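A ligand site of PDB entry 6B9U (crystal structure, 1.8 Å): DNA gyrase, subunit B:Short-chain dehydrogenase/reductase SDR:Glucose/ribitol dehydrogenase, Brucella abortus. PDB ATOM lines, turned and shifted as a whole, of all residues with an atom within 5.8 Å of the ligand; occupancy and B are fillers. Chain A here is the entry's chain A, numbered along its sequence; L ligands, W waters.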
ATOM      1  N   THR A  16       9.759  18.343  21.158  1.00  0.00           N
ATOM      2  CA  THR A  16       9.498  17.063  21.807  1.00  0.00           C
ATOM      3  C   THR A  16       9.159  17.297  23.266  1.00  0.00           C
ATOM      4  O   THR A  16       9.655  18.238  23.904  1.00  0.00           O
ATOM      5  CB  THR A  16      10.680  16.104  21.686  1.00  0.00           C
ATOM      6  OG1 THR A  16      11.804  16.613  22.411  1.00  0.00           O
ATOM      7  CG2 THR A  16      11.043  15.865  20.224  1.00  0.00           C
ATOM      8  N   GLY A  17       8.299  16.435  23.795  1.00  0.00           N
ATOM      9  CA  GLY A  17       7.894  16.577  25.179  1.00  0.00           C
ATOM     10  C   GLY A  17       7.038  17.792  25.448  1.00  0.00           C
ATOM     11  O   GLY A  17       6.988  18.264  26.588  1.00  0.00           O
ATOM     12  N   ALA A  18       6.373  18.322  24.430  1.00  0.00           N
ATOM     13  CA  ALA A  18       5.583  19.532  24.596  1.00  0.00           C
ATOM     14  C   ALA A  18       4.186  19.261  25.141  1.00  0.00           C
ATOM     15  O   ALA A  18       3.355  20.178  25.168  1.00  0.00           O
ATOM     16  CB  ALA A  18       5.502  20.296  23.275  1.00  0.00           C
ATOM     17  N   GLY A  19       3.900  18.043  25.592  1.00  0.00           N
ATOM     18  CA  GLY A  19       2.620  17.774  26.204  1.00  0.00           C
ATOM     19  C   GLY A  19       2.541  18.098  27.675  1.00  0.00           C
ATOM     20  O   GLY A  19       1.525  17.806  28.311  1.00  0.00           O
ATOM     21  N   SER A  20       3.585  18.697  28.237  1.00  0.00           N
ATOM     22  CA  SER A  20       3.690  18.946  29.664  1.00  0.00           C
ATOM     23  C   SER A  20       4.838  19.909  29.921  1.00  0.00           C
ATOM     24  O   SER A  20       5.724  20.080  29.085  1.00  0.00           O
ATOM     25  CB  SER A  20       3.912  17.621  30.420  1.00  0.00           C
ATOM     26  OG  SER A  20       4.053  17.827  31.815  1.00  0.00           O
ATOM     27  N   GLY A  21       4.794  20.559  31.090  1.00  0.00           N
ATOM     28  CA  GLY A  21       5.974  21.195  31.675  1.00  0.00           C
ATOM     29  C   GLY A  21       6.639  22.238  30.796  1.00  0.00           C
ATOM     30  O   GLY A  21       5.985  23.066  30.152  1.00  0.00           O
ATOM     31  N   PHE A  22       7.978  22.212  30.783  1.00  0.00           N
ATOM     32  CA  PHE A  22       8.734  23.198  30.020  1.00  0.00           C
ATOM     33  C   PHE A  22       8.345  23.163  28.544  1.00  0.00           C
ATOM     34  O   PHE A  22       8.198  24.210  27.901  1.00  0.00           O
ATOM     35  CB  PHE A  22      10.236  22.960  30.160  1.00  0.00           C
ATOM     36  CG  PHE A  22      10.805  23.404  31.493  1.00  0.00           C
ATOM     37  CD1 PHE A  22      10.382  24.574  32.098  1.00  0.00           C
ATOM     38  CD2 PHE A  22      11.797  22.644  32.112  1.00  0.00           C
ATOM     39  CE1 PHE A  22      10.920  24.977  33.318  1.00  0.00           C
ATOM     40  CE2 PHE A  22      12.350  23.040  33.327  1.00  0.00           C
ATOM     41  CZ  PHE A  22      11.909  24.206  33.924  1.00  0.00           C
ATOM     42  N   GLY A  23       8.190  21.963  27.983  1.00  0.00           N
ATOM     43  CA  GLY A  23       7.848  21.858  26.573  1.00  0.00           C
ATOM     44  C   GLY A  23       6.510  22.489  26.262  1.00  0.00           C
ATOM     45  O   GLY A  23       6.347  23.153  25.235  1.00  0.00           O
ATOM     46  N   VAL A  40       5.175  16.932  19.902  1.00  0.00           N
ATOM     47  CA  VAL A  40       5.554  15.520  19.840  1.00  0.00           C
ATOM     48  C   VAL A  40       5.727  15.001  21.260  1.00  0.00           C
ATOM     49  O   VAL A  40       6.560  15.516  22.013  1.00  0.00           O
ATOM     50  CB  VAL A  40       6.829  15.330  19.004  1.00  0.00           C
ATOM     51  CG1 VAL A  40       7.230  13.863  18.978  1.00  0.00           C
ATOM     52  CG2 VAL A  40       6.622  15.872  17.594  1.00  0.00           C
ATOM     53  N   ASP A  41       4.945  14.001  21.636  1.00  0.00           N
ATOM     54  CA  ASP A  41       5.014  13.504  22.996  1.00  0.00           C
ATOM     55  C   ASP A  41       4.522  12.058  23.015  1.00  0.00           C
ATOM     56  O   ASP A  41       3.714  11.652  22.184  1.00  0.00           O
ATOM     57  CB  ASP A  41       4.166  14.380  23.938  1.00  0.00           C
ATOM     58  CG  ASP A  41       4.637  14.324  25.384  1.00  0.00           C
ATOM     59  OD1 ASP A  41       4.533  13.250  26.003  1.00  0.00           O
ATOM     60  OD2 ASP A  41       5.095  15.366  25.908  1.00  0.00           O
ATOM     61  N   ARG A  42       5.059  11.265  23.949  1.00  0.00           N
ATOM     62  CA  ARG A  42       4.523   9.924  24.143  1.00  0.00           C
ATOM     63  C   ARG A  42       3.187   9.952  24.855  1.00  0.00           C
ATOM     64  O   ARG A  42       2.441   8.965  24.805  1.00  0.00           O
ATOM     65  CB  ARG A  42       5.519   9.065  24.926  1.00  0.00           C
ATOM     66  CG  ARG A  42       5.607   9.444  26.391  1.00  0.00           C
ATOM     67  CD  ARG A  42       6.678   8.656  27.134  1.00  0.00           C
ATOM     68  NE  ARG A  42       6.771   9.077  28.529  1.00  0.00           N
ATOM     69  CZ  ARG A  42       7.755   8.733  29.352  1.00  0.00           C
ATOM     70  NH1 ARG A  42       8.739   7.943  28.922  1.00  0.00           N
ATOM     71  NH2 ARG A  42       7.749   9.166  30.602  1.00  0.00           N
ATOM     72  N   ASP A  43       2.866  11.068  25.516  1.00  0.00           N
ATOM     73  CA  ASP A  43       1.629  11.257  26.260  1.00  0.00           C
ATOM     74  C   ASP A  43       0.620  11.862  25.299  1.00  0.00           C
ATOM     75  O   ASP A  43       0.564  13.075  25.113  1.00  0.00           O
ATOM     76  CB  ASP A  43       1.890  12.145  27.480  1.00  0.00           C
ATOM     77  CG  ASP A  43       0.615  12.633  28.170  1.00  0.00           C
ATOM     78  OD1 ASP A  43      -0.491  12.136  27.883  1.00  0.00           O
ATOM     79  OD2 ASP A  43       0.745  13.521  29.028  1.00  0.00           O
ATOM     80  N   ALA A  63       4.268  10.094  19.833  1.00  0.00           N
ATOM     81  CA  ALA A  63       5.442   9.355  19.394  1.00  0.00           C
ATOM     82  C   ALA A  63       6.384   9.129  20.566  1.00  0.00           C
ATOM     83  O   ALA A  63       6.518   9.987  21.434  1.00  0.00           O
ATOM     84  CB  ALA A  63       6.174  10.090  18.256  1.00  0.00           C
ATOM     85  N   ASP A  64       7.011   7.961  20.579  1.00  0.00           N
ATOM     86  CA  ASP A  64       8.076   7.630  21.520  1.00  0.00           C
ATOM     87  C   ASP A  64       9.384   7.874  20.777  1.00  0.00           C
ATOM     88  O   ASP A  64       9.794   7.059  19.940  1.00  0.00           O
ATOM     89  CB  ASP A  64       7.933   6.182  21.996  1.00  0.00           C
ATOM     90  CG  ASP A  64       9.038   5.758  22.956  1.00  0.00           C
ATOM     91  OD1 ASP A  64       9.993   6.525  23.186  1.00  0.00           O
ATOM     92  OD2 ASP A  64       8.936   4.633  23.497  1.00  0.00           O
ATOM     93  N   ILE A  65      10.033   8.995  21.081  1.00  0.00           N
ATOM     94  CA  ILE A  65      11.180   9.433  20.303  1.00  0.00           C
ATOM     95  C   ILE A  65      12.398   8.552  20.558  1.00  0.00           C
ATOM     96  O   ILE A  65      13.449   8.739  19.936  1.00  0.00           O
ATOM     97  CB  ILE A  65      11.508  10.913  20.579  1.00  0.00           C
ATOM     98  CG1 ILE A  65      12.091  11.071  21.990  1.00  0.00           C
ATOM     99  CG2 ILE A  65      10.271  11.779  20.381  1.00  0.00           C
ATOM    100  CD1 ILE A  65      12.700  12.429  22.234  1.00  0.00           C
ATOM    101  N   SER A  66      12.285   7.595  21.475  1.00  0.00           N
ATOM    102  CA  SER A  66      13.364   6.623  21.614  1.00  0.00           C
ATOM    103  C   SER A  66      13.333   5.561  20.521  1.00  0.00           C
ATOM    104  O   SER A  66      14.294   4.791  20.406  1.00  0.00           O
ATOM    105  CB  SER A  66      13.310   5.948  22.986  1.00  0.00           C
ATOM    106  OG  SER A  66      12.262   4.986  23.058  1.00  0.00           O
ATOM    107  N   ASN A  90      14.673  19.866  21.314  1.00  0.00           N
ATOM    108  CA  ASN A  90      14.811  18.547  21.942  1.00  0.00           C
ATOM    109  C   ASN A  90      14.607  18.725  23.438  1.00  0.00           C
ATOM    110  O   ASN A  90      15.545  18.967  24.197  1.00  0.00           O
ATOM    111  CB  ASN A  90      16.173  17.933  21.640  1.00  0.00           C
ATOM    112  CG  ASN A  90      16.281  17.410  20.228  1.00  0.00           C
ATOM    113  OD1 ASN A  90      15.492  16.550  19.817  1.00  0.00           O
ATOM    114  ND2 ASN A  90      17.264  17.898  19.488  1.00  0.00           N
ATOM    115  N   ASN A  91      13.351  18.583  23.876  1.00  0.00           N
ATOM    116  CA  ASN A  91      12.994  18.842  25.256  1.00  0.00           C
ATOM    117  C   ASN A  91      12.508  17.607  26.016  1.00  0.00           C
ATOM    118  O   ASN A  91      12.586  17.597  27.249  1.00  0.00           O
ATOM    119  CB  ASN A  91      11.928  19.956  25.317  1.00  0.00           C
ATOM    120  CG  ASN A  91      11.196  20.010  26.631  1.00  0.00           C
ATOM    121  OD1 ASN A  91      11.657  20.646  27.584  1.00  0.00           O
ATOM    122  ND2 ASN A  91      10.033  19.359  26.695  1.00  0.00           N
ATOM    123  N   ALA A  92      12.023  16.576  25.331  1.00  0.00           N
ATOM    124  CA  ALA A  92      11.603  15.367  26.022  1.00  0.00           C
ATOM    125  C   ALA A  92      12.758  14.800  26.849  1.00  0.00           C
ATOM    126  O   ALA A  92      13.924  14.877  26.455  1.00  0.00           O
ATOM    127  CB  ALA A  92      11.120  14.311  25.024  1.00  0.00           C
ATOM    128  N   GLY A  93      12.420  14.242  27.993  1.00  0.00           N
ATOM    129  CA  GLY A  93      13.418  13.675  28.877  1.00  0.00           C
ATOM    130  C   GLY A  93      12.749  13.009  30.056  1.00  0.00           C
ATOM    131  O   GLY A  93      11.611  13.342  30.409  1.00  0.00           O
ATOM    132  N   ILE A  94      13.462  12.050  30.647  1.00  0.00           N
ATOM    133  CA  ILE A  94      13.042  11.389  31.869  1.00  0.00           C
ATOM    134  C   ILE A  94      14.235  11.351  32.820  1.00  0.00           C
ATOM    135  O   ILE A  94      15.381  11.588  32.422  1.00  0.00           O
ATOM    136  CB  ILE A  94      12.505   9.957  31.635  1.00  0.00           C
ATOM    137  CG1 ILE A  94      13.602   9.071  31.046  1.00  0.00           C
ATOM    138  CG2 ILE A  94      11.275   9.976  30.732  1.00  0.00           C
ATOM    139  CD1 ILE A  94      13.243   7.588  31.038  1.00  0.00           C
ATOM    140  N   VAL A 115      15.748   7.811  26.077  1.00  0.00           N
ATOM    141  CA  VAL A 115      15.009   9.049  25.855  1.00  0.00           C
ATOM    142  C   VAL A 115      15.965  10.223  25.702  1.00  0.00           C
ATOM    143  O   VAL A 115      15.927  10.952  24.707  1.00  0.00           O
ATOM    144  CB  VAL A 115      13.989   9.302  26.978  1.00  0.00           C
ATOM    145  CG1 VAL A 115      13.241  10.630  26.718  1.00  0.00           C
ATOM    146  CG2 VAL A 115      13.007   8.151  27.070  1.00  0.00           C
ATOM    147  N   ASN A 116      16.827  10.429  26.698  1.00  0.00           N
ATOM    148  CA  ASN A 116      17.615  11.655  26.785  1.00  0.00           C
ATOM    149  C   ASN A 116      18.782  11.702  25.809  1.00  0.00           C
ATOM    150  O   ASN A 116      19.261  12.798  25.486  1.00  0.00           O
ATOM    151  CB  ASN A 116      18.161  11.836  28.216  1.00  0.00           C
ATOM    152  CG  ASN A 116      17.071  11.893  29.262  1.00  0.00           C
ATOM    153  OD1 ASN A 116      15.894  11.646  28.980  1.00  0.00           O
ATOM    154  ND2 ASN A 116      17.452  12.192  30.499  1.00  0.00           N
ATOM    155  N   VAL A 146      17.353  21.024  25.427  1.00  0.00           N
ATOM    156  CA  VAL A 146      17.149  21.315  26.847  1.00  0.00           C
ATOM    157  C   VAL A 146      18.026  20.372  27.652  1.00  0.00           C
ATOM    158  O   VAL A 146      17.805  19.153  27.645  1.00  0.00           O
ATOM    159  CB  VAL A 146      15.679  21.198  27.248  1.00  0.00           C
ATOM    160  CG1 VAL A 146      15.501  21.568  28.716  1.00  0.00           C
ATOM    161  CG2 VAL A 146      14.835  22.065  26.362  1.00  0.00           C
ATOM    162  N   ALA A 147      19.040  20.923  28.317  1.00  0.00           N
ATOM    163  CA  ALA A 147      19.906  20.144  29.175  1.00  0.00           C
ATOM    164  C   ALA A 147      19.504  20.372  30.631  1.00  0.00           C
ATOM    165  O   ALA A 147      18.349  20.152  30.984  1.00  0.00           O
ATOM    166  CB  ALA A 147      21.371  20.490  28.932  1.00  0.00           C
ATOM    167  N   SER A 148      20.439  20.843  31.463  1.00  0.00           N
ATOM    168  CA  SER A 148      20.198  20.999  32.899  1.00  0.00           C
ATOM    169  C   SER A 148      21.408  21.624  33.581  1.00  0.00           C
ATOM    170  O   SER A 148      22.532  21.389  33.145  1.00  0.00           O
ATOM    171  CB  SER A 148      19.901  19.647  33.550  1.00  0.00           C
ATOM    172  OG  SER A 148      19.945  19.735  34.962  1.00  0.00           O
ATOM    173  N   THR A 149      21.192  22.402  34.651  1.00  0.00           N
ATOM    174  CA  THR A 149      22.333  22.855  35.453  1.00  0.00           C
ATOM    175  C   THR A 149      23.134  21.671  36.004  1.00  0.00           C
ATOM    176  O   THR A 149      24.329  21.830  36.329  1.00  0.00           O
ATOM    177  CB  THR A 149      21.893  23.751  36.608  1.00  0.00           C
ATOM    178  OG1 THR A 149      21.037  23.030  37.495  1.00  0.00           O
ATOM    179  CG2 THR A 149      21.159  24.974  36.086  1.00  0.00           C
ATOM    180  N   TYR A 161      21.171  10.618  35.401  1.00  0.00           N
ATOM    181  CA  TYR A 161      20.383  11.649  34.756  1.00  0.00           C
ATOM    182  C   TYR A 161      21.279  12.824  34.343  1.00  0.00           C
ATOM    183  O   TYR A 161      21.273  13.237  33.182  1.00  0.00           O
ATOM    184  CB  TYR A 161      19.269  12.123  35.690  1.00  0.00           C
ATOM    185  CG  TYR A 161      18.585  13.360  35.145  1.00  0.00           C
ATOM    186  CD1 TYR A 161      17.599  13.256  34.164  1.00  0.00           C
ATOM    187  CD2 TYR A 161      18.949  14.624  35.588  1.00  0.00           C
ATOM    188  CE1 TYR A 161      16.986  14.377  33.659  1.00  0.00           C
ATOM    189  CE2 TYR A 161      18.345  15.748  35.086  1.00  0.00           C
ATOM    190  CZ  TYR A 161      17.369  15.626  34.119  1.00  0.00           C
ATOM    191  OH  TYR A 161      16.759  16.738  33.613  1.00  0.00           O
ATOM    192  N   LYS A 165      22.500  14.752  30.507  1.00  0.00           N
ATOM    193  CA  LYS A 165      22.434  16.157  30.162  1.00  0.00           C
ATOM    194  C   LYS A 165      23.815  16.696  29.805  1.00  0.00           C
ATOM    195  O   LYS A 165      23.927  17.623  28.993  1.00  0.00           O
ATOM    196  CB  LYS A 165      21.788  16.946  31.292  1.00  0.00           C
ATOM    197  CG  LYS A 165      20.324  16.559  31.533  1.00  0.00           C
ATOM    198  CD  LYS A 165      19.507  16.639  30.235  1.00  0.00           C
ATOM    199  CE  LYS A 165      18.007  16.439  30.467  1.00  0.00           C
ATOM    200  NZ  LYS A 165      17.200  16.710  29.233  1.00  0.00           N
ATOM    201  N   PRO A 191      18.228  24.709  32.395  1.00  0.00           N
ATOM    202  CA  PRO A 191      17.326  25.148  33.461  1.00  0.00           C
ATOM    203  C   PRO A 191      17.696  24.524  34.797  1.00  0.00           C
ATOM    204  O   PRO A 191      18.259  23.434  34.888  1.00  0.00           O
ATOM    205  CB  PRO A 191      15.952  24.649  32.984  1.00  0.00           C
ATOM    206  CG  PRO A 191      16.263  23.486  32.133  1.00  0.00           C
ATOM    207  CD  PRO A 191      17.573  23.763  31.469  1.00  0.00           C
ATOM    208  N   VAL A 192      17.342  25.255  35.853  1.00  0.00           N
ATOM    209  CA  VAL A 192      17.371  24.737  37.217  1.00  0.00           C
ATOM    210  C   VAL A 192      15.994  24.177  37.498  1.00  0.00           C
ATOM    211  O   VAL A 192      15.091  24.284  36.664  1.00  0.00           O
ATOM    212  CB  VAL A 192      17.772  25.845  38.220  1.00  0.00           C
ATOM    213  CG1 VAL A 192      16.601  26.799  38.453  1.00  0.00           C
ATOM    214  CG2 VAL A 192      18.282  25.258  39.517  1.00  0.00           C
ATOM    215  N   ALA A 193      15.816  23.570  38.667  1.00  0.00           N
ATOM    216  CA  ALA A 193      14.547  23.011  39.118  1.00  0.00           C
ATOM    217  C   ALA A 193      13.373  23.923  38.787  1.00  0.00           C
ATOM    218  O   ALA A 193      13.345  25.092  39.189  1.00  0.00           O
ATOM    219  CB  ALA A 193      14.601  22.761  40.623  1.00  0.00           C
ATOM    220  N   GLY A 194      12.410  23.394  38.036  1.00  0.00           N
ATOM    221  CA  GLY A 194      11.272  24.170  37.600  1.00  0.00           C
ATOM    222  C   GLY A 194       9.946  23.595  38.039  1.00  0.00           C
ATOM    223  O   GLY A 194       9.844  22.404  38.348  1.00  0.00           O
ATOM    224  N   GLU A 195       8.906  24.436  38.054  1.00  0.00           N
ATOM    225  CA  GLU A 195       7.571  24.024  38.460  1.00  0.00           C
ATOM    226  C   GLU A 195       6.908  23.320  37.283  1.00  0.00           C
ATOM    227  O   GLU A 195       6.157  23.903  36.495  1.00  0.00           O
ATOM    228  CB  GLU A 195       6.757  25.222  38.938  1.00  0.00           C
ATOM    229  N   THR A 196       7.236  22.039  37.149  1.00  0.00           N
ATOM    230  CA  THR A 196       6.675  21.137  36.156  1.00  0.00           C
ATOM    231  C   THR A 196       6.260  19.858  36.853  1.00  0.00           C
ATOM    232  O   THR A 196       6.640  19.627  38.012  1.00  0.00           O
ATOM    233  CB  THR A 196       7.697  20.811  35.049  1.00  0.00           C
ATOM    234  OG1 THR A 196       8.689  19.905  35.547  1.00  0.00           O
ATOM    235  CG2 THR A 196       8.385  22.084  34.532  1.00  0.00           C
ATOM    236  N   PRO A 197       5.458  19.001  36.201  1.00  0.00           N
ATOM    237  CA  PRO A 197       5.078  17.730  36.837  1.00  0.00           C
ATOM    238  C   PRO A 197       6.254  16.828  37.181  1.00  0.00           C
ATOM    239  O   PRO A 197       6.156  16.010  38.105  1.00  0.00           O
ATOM    240  CB  PRO A 197       4.156  17.083  35.791  1.00  0.00           C
ATOM    241  CG  PRO A 197       3.579  18.231  35.044  1.00  0.00           C
ATOM    242  CD  PRO A 197       4.666  19.276  34.984  1.00  0.00           C
ATOM    243  N   LEU A 198       7.374  16.950  36.462  1.00  0.00           N
ATOM    244  CA  LEU A 198       8.544  16.128  36.714  1.00  0.00           C
ATOM    245  C   LEU A 198       9.304  16.528  37.966  1.00  0.00           C
ATOM    246  O   LEU A 198      10.132  15.743  38.455  1.00  0.00           O
ATOM    247  CB  LEU A 198       9.489  16.194  35.504  1.00  0.00           C
ATOM    248  CG  LEU A 198      10.565  15.122  35.310  1.00  0.00           C
ATOM    249  CD1 LEU A 198       9.941  13.723  35.239  1.00  0.00           C
ATOM    250  CD2 LEU A 198      11.375  15.421  34.057  1.00  0.00           C
ATOM    251  N   LEU A 199       9.029  17.717  38.522  1.00  0.00           N
ATOM    252  CA  LEU A 199       9.810  18.224  39.652  1.00  0.00           C
ATOM    253  C   LEU A 199       9.754  17.287  40.851  1.00  0.00           C
ATOM    254  O   LEU A 199      10.767  17.104  41.549  1.00  0.00           O
ATOM    255  CB  LEU A 199       9.321  19.622  40.046  1.00  0.00           C
ATOM    256  CG  LEU A 199       9.971  20.251  41.276  1.00  0.00           C
ATOM    257  CD1 LEU A 199      11.486  20.342  41.084  1.00  0.00           C
ATOM    258  CD2 LEU A 199       9.384  21.621  41.576  1.00  0.00           C
ATOM    259  N   PHE A 202      12.601  14.617  40.612  1.00  0.00           N
ATOM    260  CA  PHE A 202      13.931  15.052  41.022  1.00  0.00           C
ATOM    261  C   PHE A 202      13.988  15.392  42.504  1.00  0.00           C
ATOM    262  O   PHE A 202      15.084  15.415  43.080  1.00  0.00           O
ATOM    263  CB  PHE A 202      14.391  16.258  40.207  1.00  0.00           C
ATOM    264  CG  PHE A 202      14.488  16.000  38.728  1.00  0.00           C
ATOM    265  CD1 PHE A 202      15.375  15.059  38.225  1.00  0.00           C
ATOM    266  CD2 PHE A 202      13.690  16.704  37.835  1.00  0.00           C
ATOM    267  CE1 PHE A 202      15.472  14.824  36.866  1.00  0.00           C
ATOM    268  CE2 PHE A 202      13.776  16.476  36.472  1.00  0.00           C
ATOM    269  CZ  PHE A 202      14.656  15.533  35.989  1.00  0.00           C
HETATM  270  P1  LIG L   1       7.540  16.974  32.174  1.00  0.00           P
HETATM  271  O1  LIG L   1       7.417  15.530  32.625  1.00  0.00           O
HETATM  272  O2  LIG L   1       6.439  17.869  32.740  1.00  0.00           O
HETATM  273  O3  LIG L   1       7.552  17.032  30.527  1.00  0.00           O
HETATM  274  C1  LIG L   1       8.345  16.073  29.858  1.00  0.00           C
HETATM  275  C2  LIG L   1       7.489  15.575  28.635  1.00  0.00           C
HETATM  276  O4  LIG L   1       8.440  14.727  27.724  1.00  0.00           O
HETATM  277  C3  LIG L   1       6.556  14.805  29.058  1.00  0.00           C
HETATM  278  O5  LIG L   1       5.223  15.249  28.614  1.00  0.00           O
HETATM  279  C4  LIG L   1       6.897  13.282  28.456  1.00  0.00           C
HETATM  280  O6  LIG L   1       5.653  12.562  28.194  1.00  0.00           O
HETATM  281  C5  LIG L   1       7.615  13.456  27.404  1.00  0.00           C
HETATM  282  N1  LIG L   1       8.496  12.271  27.298  1.00  0.00           N
HETATM  283  C6  LIG L   1       9.252  11.513  28.083  1.00  0.00           C
HETATM  284  N2  LIG L   1       9.783  10.534  27.333  1.00  0.00           N
HETATM  285  C7  LIG L   1       9.338  10.695  26.078  1.00  0.00           C
HETATM  286  C8  LIG L   1       9.595   9.937  24.951  1.00  0.00           C
HETATM  287  N3  LIG L   1      10.343   8.741  24.416  1.00  0.00           N
HETATM  288  N4  LIG L   1       9.039  10.286  23.788  1.00  0.00           N
HETATM  289  C9  LIG L   1       8.217  11.370  23.736  1.00  0.00           C
HETATM  290  N5  LIG L   1       7.964  12.129  24.854  1.00  0.00           N
HETATM  291  C10 LIG L   1       8.530  11.762  26.030  1.00  0.00           C
HETATM  292  O7  LIG L   1       8.999  17.466  32.747  1.00  0.00           O
HETATM  293  P2  LIG L   1       9.761  18.855  32.407  1.00  0.00           P
HETATM  294  O8  LIG L   1      10.200  19.419  33.733  1.00  0.00           O
HETATM  295  O9  LIG L   1       8.921  19.819  31.661  1.00  0.00           O
HETATM  296  O10 LIG L   1      11.099  18.389  31.465  1.00  0.00           O
HETATM  297  C11 LIG L   1      11.401  19.060  30.252  1.00  0.00           C
HETATM  298  C12 LIG L   1      12.947  18.962  30.055  1.00  0.00           C
HETATM  299  O11 LIG L   1      13.540  19.685  30.980  1.00  0.00           O
HETATM  300  C13 LIG L   1      13.427  17.541  30.268  1.00  0.00           C
HETATM  301  O12 LIG L   1      14.382  17.211  29.328  1.00  0.00           O
HETATM  302  C14 LIG L   1      14.060  17.579  31.666  1.00  0.00           C
HETATM  303  O13 LIG L   1      15.023  16.441  31.789  1.00  0.00           O
HETATM  304  C15 LIG L   1      14.632  18.746  31.665  1.00  0.00           C
HETATM  305  N6  LIG L   1      14.894  19.284  33.006  1.00  0.00           N
HETATM  306  C16 LIG L   1      13.812  19.373  33.983  1.00  0.00           C
HETATM  307  C17 LIG L   1      14.024  20.105  35.343  1.00  0.00           C
HETATM  308  C18 LIG L   1      12.832  20.259  36.327  1.00  0.00           C
HETATM  309  O14 LIG L   1      13.034  20.549  37.462  1.00  0.00           O
HETATM  310  N7  LIG L   1      11.434  20.043  35.855  1.00  0.00           N
HETATM  311  C19 LIG L   1      15.422  20.641  35.735  1.00  0.00           C
HETATM  312  C20 LIG L   1      16.570  20.114  34.810  1.00  0.00           C
HETATM  313  C21 LIG L   1      16.241  19.753  33.351  1.00  0.00           C
HETATM  314  O   HOH W   1       8.458  19.494  28.981  1.00  0.00           O
HETATM  315  O   HOH W   2      15.906  16.614  26.252  1.00  0.00           O
HETATM  316  O   HOH W   3       3.091  14.009  29.997  1.00  0.00           O
HETATM  317  O   HOH W   4       8.962  13.164  31.770  1.00  0.00           O
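Water W3 bridges OD2 of Asp 43 and O5 of the ligand.
Water W4 bridges an oxygen (O1) of the ligand and the backbone carbonyl oxygen of Gly 93.
N4 of the ligand lies close to O of Ala 63.
Gly 17 touches the ligand.
Gly 21 touches the ligand (CA to O9, 3.3 Å).
Asp 43 touches the ligand (CB to O6, 3.9 Å).
N of Ser 66 touches N3 of the ligand (3.7 Å).
Ala 92 touches the ligand (CA to O4, 3.6 Å).
Gly 93 touches the ligand (CA to O12, 3.7 Å).
Ile 94 touches the ligand (CG2 to C6, 3.7 Å).
Val 115 touches the ligand.
Val 146 touches the ligand (CG1 to O11, 3.5 Å).
Ala 147 touches the ligand.
Ser 148 touches the ligand (OG to C20, 3.4 Å).
Pro 191 touches the ligand.
O of Val 192 touches C19 of the ligand, at 3.8 Å.
Ala 193 touches the ligand (CA to O14, 3.3 Å).
Pro 197 touches the ligand (CD to O2, 3.2 Å).
CB of Leu 198 touches O7 of the ligand (3.1 Å).
CD1 of Leu 199 touches O14 of the ligand, 3.9 Å away.
Phe 202 touches the ligand (CE2 to C17, 3.8 Å).
Hydrophobic or aromatic side chains that line the ligand: Phe 22, Ile 65, Ala 92, Ile 94, Val 115, Val 146, Tyr 161, Pro 191, Pro 197, Leu 198, Leu 199 and Phe 202.
O of Val 40 lies within hydrogen-bond range of N of Gly 17 (2.7 Å).
N of Gly 23 sits close to ND2 of Asn 91, at 3.4 Å.
The backbone NH (N) of Leu 198 lies close to the side-chain hydroxyl (OG1) of Thr 196.
The side-chain carboxylate (OD1) of Asp 64 is in hydrogen-bond range of the side-chain hydroxyl (OG) of Ser 66 (2.7 Å).
The backbone NH of Arg 42 sits at hydrogen-bond distance from the backbone carbonyl oxygen of Ala 63 (3.2 Å).
The backbone NH (N) of Val 146 sits at hydrogen-bond distance from the backbone carbonyl oxygen (O) of Asn 90 (3.0 Å).
O of Pro 191 is in hydrogen-bond range of N of Thr 149.
OD2 of Asp 41 sits at hydrogen-bond distance from N of Gly 19 (2.9 Å).
The side-chain hydroxyl of Ser 20 sits at hydrogen-bond distance from an oxygen (O2) of the ligand, 2.6 Å away.
The guanidinium group (NH1) of Arg 42 lies within hydrogen-bond range of a nitrogen (N2) of the ligand (3.2 Å).
OD1 of Asp 41 lies within hydrogen-bond range of O6 of the ligand (2.6 Å).
N of Ile 65 lies within hydrogen-bond range of N4 of the ligand.
The backbone NH (N) of Gly 194 is in hydrogen-bond range of an oxygen (O14) of the ligand, at 3.0 Å.
N of Phe 22 lies within hydrogen-bond range of O9 of the ligand (2.7 Å).
OD1 of Asp 64 sits at hydrogen-bond distance from N3 of the ligand (2.6 Å).
An oxygen (O12) of the ligand sits at hydrogen-bond distance from the side-chain amino group of Lys 165 (2.9 Å).
A nitrogen (N5) of the ligand sits at hydrogen-bond distance from the backbone NH of Arg 42, at 3.2 Å.
The backbone carbonyl oxygen (O) of Asn 91 lies within hydrogen-bond range of an oxygen (O12) of the ligand (2.8 Å).
The side-chain hydroxyl (OH) of Tyr 161 sits at hydrogen-bond distance from an oxygen (O13) of the ligand (2.5 Å).
OG1 of Thr 196 is in hydrogen-bond range of O8 of the ligand, at 2.4 Å.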
